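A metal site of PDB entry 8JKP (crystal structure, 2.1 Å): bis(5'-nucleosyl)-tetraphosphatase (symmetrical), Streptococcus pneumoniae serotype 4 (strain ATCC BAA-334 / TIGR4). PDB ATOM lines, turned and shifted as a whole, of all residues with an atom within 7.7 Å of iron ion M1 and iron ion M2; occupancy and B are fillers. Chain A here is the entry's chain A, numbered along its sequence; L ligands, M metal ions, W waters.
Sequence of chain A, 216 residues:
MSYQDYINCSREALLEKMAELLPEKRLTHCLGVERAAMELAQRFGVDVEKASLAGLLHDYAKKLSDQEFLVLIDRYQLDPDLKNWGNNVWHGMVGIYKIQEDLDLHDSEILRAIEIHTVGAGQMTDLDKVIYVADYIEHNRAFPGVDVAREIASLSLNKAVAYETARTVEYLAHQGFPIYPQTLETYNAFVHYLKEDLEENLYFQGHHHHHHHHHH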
ATOM      1  N   ARG A  26     -27.605   9.086 -36.176  1.00  0.00           N
ATOM      2  CA  ARG A  26     -27.292   8.774 -34.772  1.00  0.00           C
ATOM      3  C   ARG A  26     -27.859   9.822 -33.798  1.00  0.00           C
ATOM      4  O   ARG A  26     -28.376   9.476 -32.730  1.00  0.00           O
ATOM      5  CB  ARG A  26     -25.771   8.597 -34.576  1.00  0.00           C
ATOM      6  CG  ARG A  26     -25.360   8.129 -33.162  1.00  0.00           C
ATOM      7  CD  ARG A  26     -26.000   6.804 -32.738  1.00  0.00           C
ATOM      8  NE  ARG A  26     -25.684   5.744 -33.690  1.00  0.00           N
ATOM      9  CZ  ARG A  26     -25.961   4.452 -33.535  1.00  0.00           C
ATOM     10  NH1 ARG A  26     -25.609   3.604 -34.490  1.00  0.00           N
ATOM     11  NH2 ARG A  26     -26.585   4.000 -32.450  1.00  0.00           N
ATOM     12  N   HIS A  29     -31.542   9.270 -33.658  1.00  0.00           N
ATOM     13  CA  HIS A  29     -31.683   8.134 -32.738  1.00  0.00           C
ATOM     14  C   HIS A  29     -31.689   8.609 -31.302  1.00  0.00           C
ATOM     15  O   HIS A  29     -32.596   8.253 -30.560  1.00  0.00           O
ATOM     16  CB  HIS A  29     -30.598   7.060 -32.968  1.00  0.00           C
ATOM     17  CG  HIS A  29     -30.507   6.023 -31.882  1.00  0.00           C
ATOM     18  ND1 HIS A  29     -31.470   5.080 -31.657  1.00  0.00           N
ATOM     19  CD2 HIS A  29     -29.520   5.772 -30.977  1.00  0.00           C
ATOM     20  CE1 HIS A  29     -31.094   4.283 -30.660  1.00  0.00           C
ATOM     21  NE2 HIS A  29     -29.902   4.673 -30.222  1.00  0.00           N
ATOM     22  N   CYS A  30     -30.713   9.432 -30.912  1.00  0.00           N
ATOM     23  CA  CYS A  30     -30.589   9.900 -29.520  1.00  0.00           C
ATOM     24  C   CYS A  30     -31.801  10.740 -29.119  1.00  0.00           C
ATOM     25  O   CYS A  30     -32.298  10.632 -27.998  1.00  0.00           O
ATOM     26  CB  CYS A  30     -29.294  10.690 -29.308  1.00  0.00           C
ATOM     27  SG  CYS A  30     -27.807   9.666 -29.302  1.00  0.00           S
ATOM     28  N   VAL A  33     -34.552   8.321 -28.474  1.00  0.00           N
ATOM     29  CA  VAL A  33     -34.375   7.672 -27.176  1.00  0.00           C
ATOM     30  C   VAL A  33     -34.766   8.645 -26.059  1.00  0.00           C
ATOM     31  O   VAL A  33     -35.399   8.240 -25.098  1.00  0.00           O
ATOM     32  CB  VAL A  33     -32.951   7.069 -26.954  1.00  0.00           C
ATOM     33  CG1 VAL A  33     -32.846   6.382 -25.600  1.00  0.00           C
ATOM     34  CG2 VAL A  33     -32.586   6.046 -28.034  1.00  0.00           C
ATOM     35  N   GLY A  55     -31.268   9.275 -21.822  1.00  0.00           N
ATOM     36  CA  GLY A  55     -31.720   8.839 -23.140  1.00  0.00           C
ATOM     37  C   GLY A  55     -31.070   9.607 -24.271  1.00  0.00           C
ATOM     38  O   GLY A  55     -30.581   9.015 -25.247  1.00  0.00           O
ATOM     39  N   HIS A  58     -27.130   8.646 -24.218  1.00  0.00           N
ATOM     40  CA  HIS A  58     -26.656   7.257 -24.074  1.00  0.00           C
ATOM     41  C   HIS A  58     -25.623   6.853 -25.160  1.00  0.00           C
ATOM     42  O   HIS A  58     -24.688   6.118 -24.864  1.00  0.00           O
ATOM     43  CB  HIS A  58     -27.811   6.263 -24.051  1.00  0.00           C
ATOM     44  CG  HIS A  58     -28.356   5.986 -25.410  1.00  0.00           C
ATOM     45  ND1 HIS A  58     -29.017   6.935 -26.144  1.00  0.00           N
ATOM     46  CD2 HIS A  58     -28.249   4.895 -26.218  1.00  0.00           C
ATOM     47  CE1 HIS A  58     -29.352   6.423 -27.315  1.00  0.00           C
ATOM     48  NE2 HIS A  58     -28.886   5.177 -27.408  1.00  0.00           N
ATOM     49  N   ASP A  59     -25.783   7.396 -26.369  1.00  0.00           N
ATOM     50  CA  ASP A  59     -24.908   7.114 -27.517  1.00  0.00           C
ATOM     51  C   ASP A  59     -23.963   8.276 -27.881  1.00  0.00           C
ATOM     52  O   ASP A  59     -23.438   8.321 -28.990  1.00  0.00           O
ATOM     53  CB  ASP A  59     -25.713   6.684 -28.753  1.00  0.00           C
ATOM     54  CG  ASP A  59     -25.987   5.177 -28.808  1.00  0.00           C
ATOM     55  OD1 ASP A  59     -25.400   4.374 -28.027  1.00  0.00           O
ATOM     56  OD2 ASP A  59     -26.865   4.731 -29.617  1.00  0.00           O
ATOM     57  N   TYR A  60     -23.754   9.207 -26.946  1.00  0.00           N
ATOM     58  CA  TYR A  60     -22.867  10.372 -27.106  1.00  0.00           C
ATOM     59  C   TYR A  60     -21.462   9.999 -27.609  1.00  0.00           C
ATOM     60  O   TYR A  60     -20.919  10.664 -28.487  1.00  0.00           O
ATOM     61  CB  TYR A  60     -22.781  11.114 -25.759  1.00  0.00           C
ATOM     62  CG  TYR A  60     -21.920  12.378 -25.727  1.00  0.00           C
ATOM     63  CD1 TYR A  60     -20.530  12.295 -25.472  1.00  0.00           C
ATOM     64  CD2 TYR A  60     -22.486  13.637 -25.912  1.00  0.00           C
ATOM     65  CE1 TYR A  60     -19.744  13.430 -25.419  1.00  0.00           C
ATOM     66  CE2 TYR A  60     -21.704  14.793 -25.858  1.00  0.00           C
ATOM     67  CZ  TYR A  60     -20.340  14.671 -25.604  1.00  0.00           C
ATOM     68  OH  TYR A  60     -19.574  15.797 -25.559  1.00  0.00           O
ATOM     69  N   LYS A  62     -20.486   7.274 -29.189  1.00  0.00           N
ATOM     70  CA  LYS A  62     -20.575   6.225 -30.208  1.00  0.00           C
ATOM     71  C   LYS A  62     -19.451   6.303 -31.260  1.00  0.00           C
ATOM     72  O   LYS A  62     -18.998   5.262 -31.731  1.00  0.00           O
ATOM     73  CB  LYS A  62     -21.952   6.240 -30.887  1.00  0.00           C
ATOM     74  CG  LYS A  62     -22.243   5.112 -31.874  1.00  0.00           C
ATOM     75  CD  LYS A  62     -22.467   3.752 -31.213  1.00  0.00           C
ATOM     76  CE  LYS A  62     -22.815   2.719 -32.270  1.00  0.00           C
ATOM     77  NZ  LYS A  62     -23.455   1.498 -31.710  1.00  0.00           N
ATOM     78  N   ASN A  87     -15.962  -1.066 -29.624  1.00  0.00           N
ATOM     79  CA  ASN A  87     -16.883   0.061 -29.558  1.00  0.00           C
ATOM     80  C   ASN A  87     -18.232  -0.323 -28.937  1.00  0.00           C
ATOM     81  O   ASN A  87     -18.765   0.427 -28.111  1.00  0.00           O
ATOM     82  CB  ASN A  87     -17.066   0.631 -30.977  1.00  0.00           C
ATOM     83  CG  ASN A  87     -17.945   1.878 -30.994  1.00  0.00           C
ATOM     84  OD1 ASN A  87     -19.158   1.802 -30.798  1.00  0.00           O
ATOM     85  ND2 ASN A  87     -17.312   3.027 -31.242  1.00  0.00           N
ATOM     86  N   ASN A  88     -18.780  -1.482 -29.359  1.00  0.00           N
ATOM     87  CA  ASN A  88     -20.056  -2.008 -28.861  1.00  0.00           C
ATOM     88  C   ASN A  88     -20.097  -2.003 -27.327  1.00  0.00           C
ATOM     89  O   ASN A  88     -21.040  -1.456 -26.736  1.00  0.00           O
ATOM     90  CB  ASN A  88     -20.350  -3.411 -29.425  1.00  0.00           C
ATOM     91  CG  ASN A  88     -20.628  -3.399 -30.940  1.00  0.00           C
ATOM     92  OD1 ASN A  88     -20.805  -2.343 -31.543  1.00  0.00           O
ATOM     93  ND2 ASN A  88     -20.682  -4.566 -31.547  1.00  0.00           N
ATOM     94  N   HIS A  91     -18.601   2.187 -25.894  1.00  0.00           N
ATOM     95  CA  HIS A  91     -19.293   3.494 -26.030  1.00  0.00           C
ATOM     96  C   HIS A  91     -20.165   3.852 -24.819  1.00  0.00           C
ATOM     97  O   HIS A  91     -20.254   5.024 -24.457  1.00  0.00           O
ATOM     98  CB  HIS A  91     -19.996   3.663 -27.393  1.00  0.00           C
ATOM     99  CG  HIS A  91     -21.308   2.938 -27.514  1.00  0.00           C
ATOM    100  ND1 HIS A  91     -21.393   1.601 -27.840  1.00  0.00           N
ATOM    101  CD2 HIS A  91     -22.593   3.369 -27.405  1.00  0.00           C
ATOM    102  CE1 HIS A  91     -22.669   1.242 -27.922  1.00  0.00           C
ATOM    103  NE2 HIS A  91     -23.437   2.300 -27.660  1.00  0.00           N
ATOM    104  N   GLY A  92     -20.757   2.841 -24.172  1.00  0.00           N
ATOM    105  CA  GLY A  92     -21.401   3.042 -22.871  1.00  0.00           C
ATOM    106  C   GLY A  92     -20.458   2.850 -21.692  1.00  0.00           C
ATOM    107  O   GLY A  92     -20.369   3.713 -20.811  1.00  0.00           O
ATOM    108  N   ILE A 114     -26.394   5.113 -18.545  1.00  0.00           N
ATOM    109  CA  ILE A 114     -25.623   5.207 -19.789  1.00  0.00           C
ATOM    110  C   ILE A 114     -24.570   4.066 -19.837  1.00  0.00           C
ATOM    111  O   ILE A 114     -24.414   3.410 -20.887  1.00  0.00           O
ATOM    112  CB  ILE A 114     -24.915   6.578 -19.970  1.00  0.00           C
ATOM    113  CG1 ILE A 114     -25.947   7.721 -20.037  1.00  0.00           C
ATOM    114  CG2 ILE A 114     -24.075   6.571 -21.252  1.00  0.00           C
ATOM    115  CD1 ILE A 114     -25.336   9.099 -19.800  1.00  0.00           C
ATOM    116  N   HIS A 117     -26.141   0.595 -20.799  1.00  0.00           N
ATOM    117  CA  HIS A 117     -27.256   0.684 -21.765  1.00  0.00           C
ATOM    118  C   HIS A 117     -27.192  -0.403 -22.853  1.00  0.00           C
ATOM    119  O   HIS A 117     -28.230  -0.782 -23.379  1.00  0.00           O
ATOM    120  CB  HIS A 117     -27.404   2.098 -22.372  1.00  0.00           C
ATOM    121  CG  HIS A 117     -26.553   2.344 -23.583  1.00  0.00           C
ATOM    122  ND1 HIS A 117     -25.313   2.915 -23.501  1.00  0.00           N
ATOM    123  CD2 HIS A 117     -26.783   2.104 -24.902  1.00  0.00           C
ATOM    124  CE1 HIS A 117     -24.788   2.998 -24.715  1.00  0.00           C
ATOM    125  NE2 HIS A 117     -25.668   2.523 -25.605  1.00  0.00           N
ATOM    126  N   THR A 118     -26.001  -0.907 -23.158  1.00  0.00           N
ATOM    127  CA  THR A 118     -25.822  -1.955 -24.187  1.00  0.00           C
ATOM    128  C   THR A 118     -25.914  -3.351 -23.555  1.00  0.00           C
ATOM    129  O   THR A 118     -26.635  -4.203 -24.053  1.00  0.00           O
ATOM    130  CB  THR A 118     -24.467  -1.817 -24.929  1.00  0.00           C
ATOM    131  OG1 THR A 118     -24.326  -0.491 -25.425  1.00  0.00           O
ATOM    132  CG2 THR A 118     -24.310  -2.818 -26.084  1.00  0.00           C
ATOM    133  N   ILE A 131     -33.695   3.218 -19.864  1.00  0.00           N
ATOM    134  CA  ILE A 131     -32.764   3.578 -20.936  1.00  0.00           C
ATOM    135  C   ILE A 131     -32.524   2.379 -21.865  1.00  0.00           C
ATOM    136  O   ILE A 131     -32.590   2.521 -23.091  1.00  0.00           O
ATOM    137  CB  ILE A 131     -31.445   4.154 -20.378  1.00  0.00           C
ATOM    138  CG1 ILE A 131     -31.736   5.374 -19.477  1.00  0.00           C
ATOM    139  CG2 ILE A 131     -30.461   4.502 -21.512  1.00  0.00           C
ATOM    140  CD1 ILE A 131     -32.714   6.390 -20.064  1.00  0.00           C
ATOM    141  N   ALA A 134     -35.758   1.942 -23.882  1.00  0.00           N
ATOM    142  CA  ALA A 134     -35.984   3.133 -24.740  1.00  0.00           C
ATOM    143  C   ALA A 134     -35.114   3.118 -25.993  1.00  0.00           C
ATOM    144  O   ALA A 134     -35.588   3.472 -27.086  1.00  0.00           O
ATOM    145  CB  ALA A 134     -35.735   4.418 -23.954  1.00  0.00           C
ATOM    146  N   ASP A 135     -33.859   2.706 -25.809  1.00  0.00           N
ATOM    147  CA  ASP A 135     -32.867   2.509 -26.879  1.00  0.00           C
ATOM    148  C   ASP A 135     -33.400   1.600 -28.004  1.00  0.00           C
ATOM    149  O   ASP A 135     -33.219   1.880 -29.203  1.00  0.00           O
ATOM    150  CB  ASP A 135     -31.603   1.906 -26.255  1.00  0.00           C
ATOM    151  CG  ASP A 135     -30.429   1.854 -27.215  1.00  0.00           C
ATOM    152  OD1 ASP A 135     -30.276   2.717 -28.145  1.00  0.00           O
ATOM    153  OD2 ASP A 135     -29.593   0.956 -27.012  1.00  0.00           O
ATOM    154  N   TYR A 136     -34.066   0.527 -27.581  1.00  0.00           N
ATOM    155  CA  TYR A 136     -34.560  -0.546 -28.452  1.00  0.00           C
ATOM    156  C   TYR A 136     -35.854  -0.164 -29.150  1.00  0.00           C
ATOM    157  O   TYR A 136     -36.085  -0.578 -30.285  1.00  0.00           O
ATOM    158  CB  TYR A 136     -34.808  -1.797 -27.601  1.00  0.00           C
ATOM    159  CG  TYR A 136     -34.767  -3.135 -28.306  1.00  0.00           C
ATOM    160  CD1 TYR A 136     -33.649  -3.538 -29.068  1.00  0.00           C
ATOM    161  CD2 TYR A 136     -35.834  -4.052 -28.170  1.00  0.00           C
ATOM    162  CE1 TYR A 136     -33.607  -4.782 -29.685  1.00  0.00           C
ATOM    163  CE2 TYR A 136     -35.788  -5.306 -28.777  1.00  0.00           C
ATOM    164  CZ  TYR A 136     -34.681  -5.652 -29.525  1.00  0.00           C
ATOM    165  OH  TYR A 136     -34.631  -6.877 -30.139  1.00  0.00           O
ATOM    166  N   GLU A 138     -37.346   3.144 -29.495  1.00  0.00           N
ATOM    167  CA  GLU A 138     -37.512   4.524 -29.986  1.00  0.00           C
ATOM    168  C   GLU A 138     -38.072   4.542 -31.421  1.00  0.00           C
ATOM    169  O   GLU A 138     -37.766   3.652 -32.226  1.00  0.00           O
ATOM    170  CB  GLU A 138     -36.215   5.337 -29.853  1.00  0.00           C
ATOM    171  CG  GLU A 138     -35.051   4.853 -30.713  1.00  0.00           C
ATOM    172  CD  GLU A 138     -34.931   5.586 -32.050  1.00  0.00           C
ATOM    173  OE1 GLU A 138     -35.772   6.474 -32.347  1.00  0.00           O
ATOM    174  OE2 GLU A 138     -33.966   5.282 -32.788  1.00  0.00           O
ATOM    175  N   ARG A 141     -36.584   3.298 -34.857  1.00  0.00           N
ATOM    176  CA  ARG A 141     -36.201   1.900 -35.168  1.00  0.00           C
ATOM    177  C   ARG A 141     -37.298   1.154 -35.928  1.00  0.00           C
ATOM    178  O   ARG A 141     -38.474   1.371 -35.696  1.00  0.00           O
ATOM    179  CB  ARG A 141     -35.849   1.090 -33.927  1.00  0.00           C
ATOM    180  CG  ARG A 141     -35.101   1.799 -32.822  1.00  0.00           C
ATOM    181  CD  ARG A 141     -33.584   1.724 -32.947  1.00  0.00           C
ATOM    182  NE  ARG A 141     -33.045   0.402 -33.282  1.00  0.00           N
ATOM    183  CZ  ARG A 141     -32.265  -0.332 -32.487  1.00  0.00           C
ATOM    184  NH1 ARG A 141     -31.809  -1.498 -32.919  1.00  0.00           N
ATOM    185  NH2 ARG A 141     -31.940   0.088 -31.273  1.00  0.00           N
HETATM  186  P1  LIG L   1     -26.543  -0.664 -28.564  1.00  0.00           P
HETATM  187  O1  LIG L   1     -27.554  -1.481 -27.774  1.00  0.00           O
HETATM  188  O2  LIG L   1     -25.634   0.216 -27.697  1.00  0.00           O
HETATM  189  O3  LIG L   1     -27.167   0.076 -29.734  1.00  0.00           O
HETATM  190  O4  LIG L   1     -25.613  -1.825 -29.180  1.00  0.00           O
HETATM  191  C1  LIG L   1     -24.793  -1.632 -30.323  1.00  0.00           C
HETATM  192  C2  LIG L   1     -24.282  -2.980 -30.833  1.00  0.00           C
HETATM  193  O5  LIG L   1     -23.579  -3.680 -29.801  1.00  0.00           O
HETATM  194  C3  LIG L   1     -25.377  -3.895 -31.337  1.00  0.00           C
HETATM  195  O6  LIG L   1     -25.221  -4.031 -32.738  1.00  0.00           O
HETATM  196  C4  LIG L   1     -25.128  -5.254 -30.698  1.00  0.00           C
HETATM  197  C5  LIG L   1     -23.779  -5.074 -29.999  1.00  0.00           C
HETATM  198  N1  LIG L   1     -23.635  -5.843 -28.750  1.00  0.00           N
HETATM  199  C6  LIG L   1     -22.446  -6.601 -28.623  1.00  0.00           C
HETATM  200  O7  LIG L   1     -21.598  -6.565 -29.530  1.00  0.00           O
HETATM  201  N2  LIG L   1     -22.171  -7.360 -27.569  1.00  0.00           N
HETATM  202  C7  LIG L   1     -23.037  -7.415 -26.571  1.00  0.00           C
HETATM  203  O8  LIG L   1     -22.740  -8.127 -25.615  1.00  0.00           O
HETATM  204  C8  LIG L   1     -24.317  -6.635 -26.660  1.00  0.00           C
HETATM  205  C9  LIG L   1     -25.354  -6.657 -25.579  1.00  0.00           C
HETATM  206  C10 LIG L   1     -24.570  -5.866 -27.793  1.00  0.00           C
HETATM  207 FE    FE M   1     -28.656   3.815 -28.917  1.00  0.00          FE
HETATM  208 FE    FE M   2     -25.469   2.330 -27.590  1.00  0.00          FE
HETATM  209  O   HOH W   1     -25.254   2.313 -29.610  1.00  0.00           O
HETATM  210  O   HOH W   2     -27.494   2.483 -27.927  1.00  0.00           O
HETATM  211  O   HOH W   3     -28.630   2.403 -30.410  1.00  0.00           O
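OG1 of Thr 118 lies close to O2 of the ligand, at 2.7 Å. The side-chain amide nitrogen of Asn 88 lies within hydrogen-bond range of an oxygen (O7) of the ligand (3.0 Å).
ND1 of His 29 sits at hydrogen-bond distance from OE2 of Glu 138 (2.7 Å). NE2 of His 117 lies close to OG1 of Thr 118 (3.3 Å). The backbone carbonyl oxygen of Ile 114 is in hydrogen-bond range of a ring nitrogen (ND1) of His 117 (2.8 Å). A ring nitrogen (ND1) of His 91 is in hydrogen-bond range of the backbone carbonyl oxygen of Asn 88 (3.3 Å). O of Asn 87 lies within hydrogen-bond range of ND1 of His 91, 2.9 Å away. A ring nitrogen (ND1) of His 58 sits at hydrogen-bond distance from the backbone carbonyl oxygen of Gly 55 (2.8 Å). The side-chain carboxylate of Asp 59 sits close to the guanidinium group of Arg 26 (2.9 Å). The backbone carbonyl oxygen of Asp 135 sits at hydrogen-bond distance from the guanidinium group of Arg 141 (3.0 Å).
The nearest printed residue that does not touch iron ion M1 is Arg 26 (4.1 Å).
Merely in contact with iron ion M2: Thr 118. Within 4 Å of iron ion M2: Asp 59, His 91, His 117 and Thr 118.
Iron ion M1 is bound by NE2 of His 29 (2.0 Å), water W2 (2.0 Å), NE2 of His 58 (2.0 Å), water W3 (2.1 Å), OD1 of Asp 135 (2.1 Å) and OD2 of Asp 59 (2.1 Å). Iron ion M1 has six donor atoms within binding distance.
Iron ion M2 is bound by NE2 of His 117 (2.0 Å). Iron ion M2 is bound by water W1 (2.0 Å). NE2 of His 91 is bound to iron ion M2. Iron ion M2 is bound by water W2. The side-chain carboxylate (OD1) of Asp 59 binds iron ion M2. An oxygen (O2) of the ligand binds iron ion M2 (2.1 Å). Iron ion M2 has six donor atoms within binding distance.
Water W3 bridges O3 of the ligand (2.8 Å) and NH2 of Arg 26 (3.3 Å). Water W2 lies within hydrogen-bond range of OD2 of Asp 135 and O3 of the ligand. Water W1 lies within hydrogen-bond range of the side-chain amino group of Lys 62 (2.9 Å) and an oxygen (O3) of the ligand (2.9 Å).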
